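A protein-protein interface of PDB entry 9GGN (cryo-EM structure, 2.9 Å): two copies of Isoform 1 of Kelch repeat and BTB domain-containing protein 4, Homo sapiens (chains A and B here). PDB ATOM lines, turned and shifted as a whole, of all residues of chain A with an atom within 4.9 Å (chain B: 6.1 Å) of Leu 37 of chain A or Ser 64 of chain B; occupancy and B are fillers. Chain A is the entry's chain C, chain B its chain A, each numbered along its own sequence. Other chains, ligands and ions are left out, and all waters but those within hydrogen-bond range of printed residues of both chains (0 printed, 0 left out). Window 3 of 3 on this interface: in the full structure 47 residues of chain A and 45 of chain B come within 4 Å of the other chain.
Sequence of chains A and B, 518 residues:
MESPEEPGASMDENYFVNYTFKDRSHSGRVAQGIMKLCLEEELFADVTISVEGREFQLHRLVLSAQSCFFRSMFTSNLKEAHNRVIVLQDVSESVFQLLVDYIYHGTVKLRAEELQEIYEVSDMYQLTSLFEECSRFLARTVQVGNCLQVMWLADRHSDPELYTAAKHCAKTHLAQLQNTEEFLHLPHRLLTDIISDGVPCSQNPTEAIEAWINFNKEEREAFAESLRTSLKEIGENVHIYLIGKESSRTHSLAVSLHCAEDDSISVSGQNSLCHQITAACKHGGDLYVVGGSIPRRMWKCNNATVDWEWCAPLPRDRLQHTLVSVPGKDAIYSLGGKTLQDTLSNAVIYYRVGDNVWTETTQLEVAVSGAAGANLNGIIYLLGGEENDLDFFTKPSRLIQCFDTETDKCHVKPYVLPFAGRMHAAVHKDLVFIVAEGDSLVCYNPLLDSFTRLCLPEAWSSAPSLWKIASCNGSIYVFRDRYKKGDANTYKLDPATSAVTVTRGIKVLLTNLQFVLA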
ATOM      1  N   GLY A  33       2.071   0.802  21.714  1.00  0.00           N
ATOM      2  CA  GLY A  33       2.549   1.509  22.891  1.00  0.00           C
ATOM      3  C   GLY A  33       4.058   1.467  23.027  1.00  0.00           C
ATOM      4  O   GLY A  33       4.682   2.453  23.427  1.00  0.00           O
ATOM      5  N   ILE A  34       4.665   0.323  22.705  1.00  0.00           N
ATOM      6  CA  ILE A  34       6.122   0.225  22.717  1.00  0.00           C
ATOM      7  C   ILE A  34       6.726   1.200  21.713  1.00  0.00           C
ATOM      8  O   ILE A  34       7.659   1.944  22.030  1.00  0.00           O
ATOM      9  CB  ILE A  34       6.578  -1.222  22.452  1.00  0.00           C
ATOM     10  CG1 ILE A  34       6.577  -2.061  23.741  1.00  0.00           C
ATOM     11  CG2 ILE A  34       7.961  -1.248  21.815  1.00  0.00           C
ATOM     12  CD1 ILE A  34       5.294  -2.058  24.541  1.00  0.00           C
ATOM     13  N   MET A  35       6.185   1.230  20.494  1.00  0.00           N
ATOM     14  CA  MET A  35       6.713   2.138  19.480  1.00  0.00           C
ATOM     15  C   MET A  35       6.578   3.592  19.916  1.00  0.00           C
ATOM     16  O   MET A  35       7.489   4.401  19.705  1.00  0.00           O
ATOM     17  CB  MET A  35       6.001   1.908  18.146  1.00  0.00           C
ATOM     18  N   LYS A  36       5.445   3.943  20.527  1.00  0.00           N
ATOM     19  CA  LYS A  36       5.177   5.336  20.866  1.00  0.00           C
ATOM     20  C   LYS A  36       5.991   5.821  22.061  1.00  0.00           C
ATOM     21  O   LYS A  36       6.289   7.017  22.151  1.00  0.00           O
ATOM     22  CB  LYS A  36       3.685   5.528  21.138  1.00  0.00           C
ATOM     23  N   LEU A  37       6.365   4.931  22.983  1.00  0.00           N
ATOM     24  CA  LEU A  37       6.991   5.355  24.231  1.00  0.00           C
ATOM     25  C   LEU A  37       8.499   5.113  24.277  1.00  0.00           C
ATOM     26  O   LEU A  37       9.088   5.157  25.362  1.00  0.00           O
ATOM     27  CB  LEU A  37       6.313   4.664  25.416  1.00  0.00           C
ATOM     28  CG  LEU A  37       5.087   5.355  26.021  1.00  0.00           C
ATOM     29  CD1 LEU A  37       3.939   5.444  25.027  1.00  0.00           C
ATOM     30  CD2 LEU A  37       4.643   4.642  27.290  1.00  0.00           C
ATOM     31  N   CYS A  38       9.138   4.854  23.136  1.00  0.00           N
ATOM     32  CA  CYS A  38      10.599   4.828  23.072  1.00  0.00           C
ATOM     33  C   CYS A  38      11.119   5.873  22.093  1.00  0.00           C
ATOM     34  O   CYS A  38      11.823   6.793  22.515  1.00  0.00           O
ATOM     35  CB  CYS A  38      11.132   3.433  22.744  1.00  0.00           C
ATOM     36  SG  CYS A  38      10.198   2.061  23.439  1.00  0.00           S
ATOM     37  N   LEU A  39      10.819   5.751  20.794  1.00  0.00           N
ATOM     38  CA  LEU A  39      11.309   6.726  19.823  1.00  0.00           C
ATOM     39  C   LEU A  39      10.907   8.150  20.185  1.00  0.00           C
ATOM     40  O   LEU A  39      11.565   9.100  19.750  1.00  0.00           O
ATOM     41  CB  LEU A  39      10.798   6.378  18.423  1.00  0.00           C
ATOM     42  CG  LEU A  39      11.277   5.040  17.857  1.00  0.00           C
ATOM     43  CD1 LEU A  39      10.625   4.757  16.513  1.00  0.00           C
ATOM     44  CD2 LEU A  39      12.794   5.022  17.739  1.00  0.00           C
ATOM     45  N   GLU A  40       9.844   8.316  20.968  1.00  0.00           N
ATOM     46  CA  GLU A  40       9.445   9.607  21.503  1.00  0.00           C
ATOM     47  C   GLU A  40       9.273   9.458  23.005  1.00  0.00           C
ATOM     48  O   GLU A  40       8.775   8.431  23.477  1.00  0.00           O
ATOM     49  CB  GLU A  40       8.145  10.108  20.862  1.00  0.00           C
ATOM     50  N   GLU A  41       9.695  10.480  23.754  1.00  0.00           N
ATOM     51  CA  GLU A  41       9.541  10.502  25.209  1.00  0.00           C
ATOM     52  C   GLU A  41      10.282   9.321  25.842  1.00  0.00           C
ATOM     53  O   GLU A  41       9.714   8.528  26.595  1.00  0.00           O
ATOM     54  CB  GLU A  41       8.059  10.521  25.603  1.00  0.00           C
ATOM     55  CG  GLU A  41       7.779  10.772  27.082  1.00  0.00           C
ATOM     56  CD  GLU A  41       6.321  10.565  27.438  1.00  0.00           C
ATOM     57  OE1 GLU A  41       5.506  10.358  26.514  1.00  0.00           O
ATOM     58  OE2 GLU A  41       5.989  10.609  28.641  1.00  0.00           O
ATOM     59  N   GLU A  42      11.557   9.183  25.476  1.00  0.00           N
ATOM     60  CA  GLU A  42      12.389   8.083  25.959  1.00  0.00           C
ATOM     61  C   GLU A  42      12.294   7.940  27.472  1.00  0.00           C
ATOM     62  O   GLU A  42      12.465   8.910  28.215  1.00  0.00           O
ATOM     63  CB  GLU A  42      13.844   8.308  25.542  1.00  0.00           C
ATOM     64  N   LEU A  43      12.034   6.713  27.925  1.00  0.00           N
ATOM     65  CA  LEU A  43      11.871   6.430  29.342  1.00  0.00           C
ATOM     66  C   LEU A  43      12.259   4.983  29.614  1.00  0.00           C
ATOM     67  O   LEU A  43      12.221   4.133  28.722  1.00  0.00           O
ATOM     68  CB  LEU A  43      10.430   6.683  29.806  1.00  0.00           C
ATOM     69  CG  LEU A  43       9.974   8.123  30.043  1.00  0.00           C
ATOM     70  CD1 LEU A  43       8.457   8.195  30.120  1.00  0.00           C
ATOM     71  CD2 LEU A  43      10.604   8.684  31.308  1.00  0.00           C
ATOM     72  N   PHE A  44      12.617   4.717  30.871  1.00  0.00           N
ATOM     73  CA  PHE A  44      12.980   3.373  31.331  1.00  0.00           C
ATOM     74  C   PHE A  44      14.073   2.756  30.462  1.00  0.00           C
ATOM     75  O   PHE A  44      14.036   1.570  30.129  1.00  0.00           O
ATOM     76  CB  PHE A  44      11.755   2.458  31.385  1.00  0.00           C
ATOM     77  CG  PHE A  44      10.494   3.153  31.806  1.00  0.00           C
ATOM     78  CD1 PHE A  44      10.250   3.426  33.140  1.00  0.00           C
ATOM     79  CD2 PHE A  44       9.539   3.514  30.869  1.00  0.00           C
ATOM     80  CE1 PHE A  44       9.089   4.062  33.531  1.00  0.00           C
ATOM     81  CE2 PHE A  44       8.375   4.150  31.254  1.00  0.00           C
ATOM     82  CZ  PHE A  44       8.150   4.424  32.587  1.00  0.00           C
ATOM     83  N   HIS A  59      16.258   0.816  25.293  1.00  0.00           N
ATOM     84  CA  HIS A  59      15.603   0.086  26.367  1.00  0.00           C
ATOM     85  C   HIS A  59      15.948  -1.397  26.296  1.00  0.00           C
ATOM     86  O   HIS A  59      16.105  -1.965  25.213  1.00  0.00           O
ATOM     87  CB  HIS A  59      14.090   0.279  26.304  1.00  0.00           C
ATOM     88  CG  HIS A  59      13.659   1.711  26.225  1.00  0.00           C
ATOM     89  ND1 HIS A  59      14.545   2.765  26.293  1.00  0.00           N
ATOM     90  CD2 HIS A  59      12.430   2.262  26.089  1.00  0.00           C
ATOM     91  CE1 HIS A  59      13.882   3.903  26.197  1.00  0.00           C
ATOM     92  NE2 HIS A  59      12.596   3.626  26.074  1.00  0.00           N
ATOM     93  N   ARG B  60       9.299  -2.848  33.793  1.00  0.00           N
ATOM     94  CA  ARG B  60       8.752  -1.500  33.693  1.00  0.00           C
ATOM     95  C   ARG B  60       8.186  -1.225  32.305  1.00  0.00           C
ATOM     96  O   ARG B  60       7.033  -0.801  32.172  1.00  0.00           O
ATOM     97  CB  ARG B  60       9.828  -0.470  34.038  1.00  0.00           C
ATOM     98  N   LEU B  61       8.997  -1.442  31.265  1.00  0.00           N
ATOM     99  CA  LEU B  61       8.623  -1.048  29.909  1.00  0.00           C
ATOM    100  C   LEU B  61       7.274  -1.619  29.491  1.00  0.00           C
ATOM    101  O   LEU B  61       6.455  -0.915  28.890  1.00  0.00           O
ATOM    102  CB  LEU B  61       9.714  -1.476  28.925  1.00  0.00           C
ATOM    103  CG  LEU B  61       9.499  -1.045  27.473  1.00  0.00           C
ATOM    104  CD1 LEU B  61      10.820  -0.674  26.861  1.00  0.00           C
ATOM    105  CD2 LEU B  61       8.843  -2.153  26.656  1.00  0.00           C
ATOM    106  N   VAL B  62       7.039  -2.909  29.756  1.00  0.00           N
ATOM    107  CA  VAL B  62       5.779  -3.523  29.341  1.00  0.00           C
ATOM    108  C   VAL B  62       4.594  -2.768  29.937  1.00  0.00           C
ATOM    109  O   VAL B  62       3.679  -2.350  29.217  1.00  0.00           O
ATOM    110  CB  VAL B  62       5.754  -5.025  29.687  1.00  0.00           C
ATOM    111  CG1 VAL B  62       6.863  -5.736  28.954  1.00  0.00           C
ATOM    112  CG2 VAL B  62       5.921  -5.261  31.179  1.00  0.00           C
ATOM    113  N   LEU B  63       4.585  -2.589  31.255  1.00  0.00           N
ATOM    114  CA  LEU B  63       3.575  -1.742  31.858  1.00  0.00           C
ATOM    115  C   LEU B  63       3.743  -0.304  31.368  1.00  0.00           C
ATOM    116  O   LEU B  63       4.741   0.060  30.743  1.00  0.00           O
ATOM    117  CB  LEU B  63       3.661  -1.808  33.380  1.00  0.00           C
ATOM    118  CG  LEU B  63       3.334  -3.175  33.983  1.00  0.00           C
ATOM    119  CD1 LEU B  63       3.801  -3.256  35.428  1.00  0.00           C
ATOM    120  CD2 LEU B  63       1.850  -3.493  33.866  1.00  0.00           C
ATOM    121  N   SER B  64       2.722   0.506  31.644  1.00  0.00           N
ATOM    122  CA  SER B  64       2.615   1.896  31.204  1.00  0.00           C
ATOM    123  C   SER B  64       2.349   1.988  29.705  1.00  0.00           C
ATOM    124  O   SER B  64       1.802   2.988  29.229  1.00  0.00           O
ATOM    125  CB  SER B  64       3.869   2.695  31.572  1.00  0.00           C
ATOM    126  N   ALA B  65       2.731   0.954  28.951  1.00  0.00           N
ATOM    127  CA  ALA B  65       2.461   0.914  27.521  1.00  0.00           C
ATOM    128  C   ALA B  65       1.038   0.481  27.208  1.00  0.00           C
ATOM    129  O   ALA B  65       0.634   0.520  26.040  1.00  0.00           O
ATOM    130  CB  ALA B  65       3.451  -0.020  26.824  1.00  0.00           C
ATOM    131  N   GLN B  66       0.291   0.063  28.206  1.00  0.00           N
ATOM    132  CA  GLN B  66      -1.114  -0.305  28.116  1.00  0.00           C
ATOM    133  C   GLN B  66      -1.955   0.381  29.177  1.00  0.00           C
ATOM    134  O   GLN B  66      -3.105   0.739  28.910  1.00  0.00           O
ATOM    135  CB  GLN B  66      -1.272  -1.829  28.227  1.00  0.00           C
ATOM    136  N   SER B  67      -1.407   0.572  30.374  1.00  0.00           N
ATOM    137  CA  SER B  67      -2.074   1.279  31.460  1.00  0.00           C
ATOM    138  C   SER B  67      -1.399   2.629  31.662  1.00  0.00           C
ATOM    139  O   SER B  67      -0.245   2.693  32.097  1.00  0.00           O
ATOM    140  CB  SER B  67      -2.015   0.450  32.741  1.00  0.00           C
ATOM    141  N   CYS B  68      -2.124   3.711  31.364  1.00  0.00           N
ATOM    142  CA  CYS B  68      -1.545   5.039  31.525  1.00  0.00           C
ATOM    143  C   CYS B  68      -1.336   5.378  32.995  1.00  0.00           C
ATOM    144  O   CYS B  68      -0.467   6.198  33.326  1.00  0.00           O
ATOM    145  CB  CYS B  68      -2.434   6.087  30.855  1.00  0.00           C
ATOM    146  N   PHE B  70       0.017   3.559  35.128  1.00  0.00           N
ATOM    147  CA  PHE B  70       1.383   3.171  35.463  1.00  0.00           C
ATOM    148  C   PHE B  70       2.409   4.066  34.788  1.00  0.00           C
ATOM    149  O   PHE B  70       3.533   4.185  35.288  1.00  0.00           O
ATOM    150  CB  PHE B  70       1.651   1.714  35.073  1.00  0.00           C
ATOM    151  CG  PHE B  70       0.963   0.701  35.949  1.00  0.00           C
ATOM    152  CD1 PHE B  70       0.046   1.090  36.907  1.00  0.00           C
ATOM    153  CD2 PHE B  70       1.249  -0.646  35.815  1.00  0.00           C
ATOM    154  CE1 PHE B  70      -0.578   0.154  37.710  1.00  0.00           C
ATOM    155  CE2 PHE B  70       0.627  -1.586  36.613  1.00  0.00           C
ATOM    156  CZ  PHE B  70      -0.287  -1.185  37.563  1.00  0.00           C
ATOM    157  N   ARG B  71       2.032   4.735  33.700  1.00  0.00           N
ATOM    158  CA  ARG B  71       2.890   5.770  33.140  1.00  0.00           C
ATOM    159  C   ARG B  71       3.025   6.921  34.126  1.00  0.00           C
ATOM    160  O   ARG B  71       4.131   7.256  34.563  1.00  0.00           O
ATOM    161  CB  ARG B  71       2.332   6.255  31.800  1.00  0.00           C
ATOM    162  N   SER B  72       1.899   7.550  34.469  1.00  0.00           N
ATOM    163  CA  SER B  72       1.858   8.544  35.537  1.00  0.00           C
ATOM    164  C   SER B  72       2.615   8.073  36.776  1.00  0.00           C
ATOM    165  O   SER B  72       3.367   8.844  37.381  1.00  0.00           O
ATOM    166  CB  SER B  72       0.408   8.875  35.900  1.00  0.00           C
ATOM    167  N   PHE B  74       5.092   5.965  36.995  1.00  0.00           N
ATOM    168  CA  PHE B  74       6.528   5.781  36.813  1.00  0.00           C
ATOM    169  C   PHE B  74       7.150   6.889  35.971  1.00  0.00           C
ATOM    170  O   PHE B  74       7.946   6.615  35.068  1.00  0.00           O
ATOM    171  CB  PHE B  74       6.816   4.420  36.173  1.00  0.00           C
ATOM    172  CG  PHE B  74       6.175   3.259  36.883  1.00  0.00           C
ATOM    173  CD1 PHE B  74       6.010   3.270  38.258  1.00  0.00           C
ATOM    174  CD2 PHE B  74       5.745   2.153  36.171  1.00  0.00           C
ATOM    175  CE1 PHE B  74       5.421   2.201  38.907  1.00  0.00           C
ATOM    176  CE2 PHE B  74       5.156   1.082  36.814  1.00  0.00           C
ATOM    177  CZ  PHE B  74       4.994   1.106  38.184  1.00  0.00           C
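No position is printed for both chains. Of the 6 pairs that touch across the chains among the printed residues, none has its exchanged pair printed and touching as well.
Of the printed residues of chain B, Leu 37 of chain A touches Ser 64 (3.8 Å). Ser 64 of chain B touches just one residue of chain A: Leu 37. Of the printed residues of chain B, Gly 33 of chain A touches Ala 65. Printed residues of chain B within 4 Å of Ile 34 of chain A: Leu 61 (3.7 Å) and Ala 65 (3.6 Å). Val 62 of chain B touches none of the printed residues of chain A. Leu 39 of chain A touches none of the printed residues of chain B. The nearest residue of chain B that does not touch Leu 37 of chain A is Ala 65 of chain B (4.3 Å). The nearest residue of chain A that does not touch Ser 64 of chain B is Phe 44 of chain A (4.7 Å). The nearest printed residue of chain A that does not touch Leu 61 of chain B is Cys 38 of chain A (4.4 Å).
Of the 13 printed residues of chain B, 4 touch a printed residue of chain A. Hydrophobic or aromatic side chains of chain B within 4 Å of the printed part of chain A: Leu 61, Ala 65 and Phe 74. Of the 13 printed residues of chain A, 5 touch a printed residue of chain B. Hydrophobic or aromatic side chains of chain A that line the printed part of chain B: Ile 34, Leu 37, Phe 44 and His 59. Along chain A the printed residues that touch a printed residue of chain B span positions 33 to 59. Among the printed residues, 6 pairs touch across the chains. Among the printed residues, no Asp or Glu carboxylate lies within 4 Å of a Lys or Arg side-chain nitrogen of the other chain.
Ala 65 of chain B touches Gly 33 of chain A (O to CA, 3.8 Å). CD2 of Leu 61 of chain B touches CG1 of Ile 34 of chain A (3.7 Å). CB of Ala 65 of chain B touches CD1 of Ile 34 of chain A (3.6 Å). Leu 37 of chain A touches Ser 64 of chain B. O of Phe 74 of chain B touches CE1 of Phe 44 of chain A, at 3.2 Å. His 59 of chain A touches Leu 61 of chain B (CD2 to CD1, 3.4 Å).
O of Ile 34 of chain A is in hydrogen-bond range of SG of Cys 38 of chain A (2.9 Å). O of Leu 43 of chain A is in hydrogen-bond range of NE2 of His 59 of chain A (2.7 Å).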
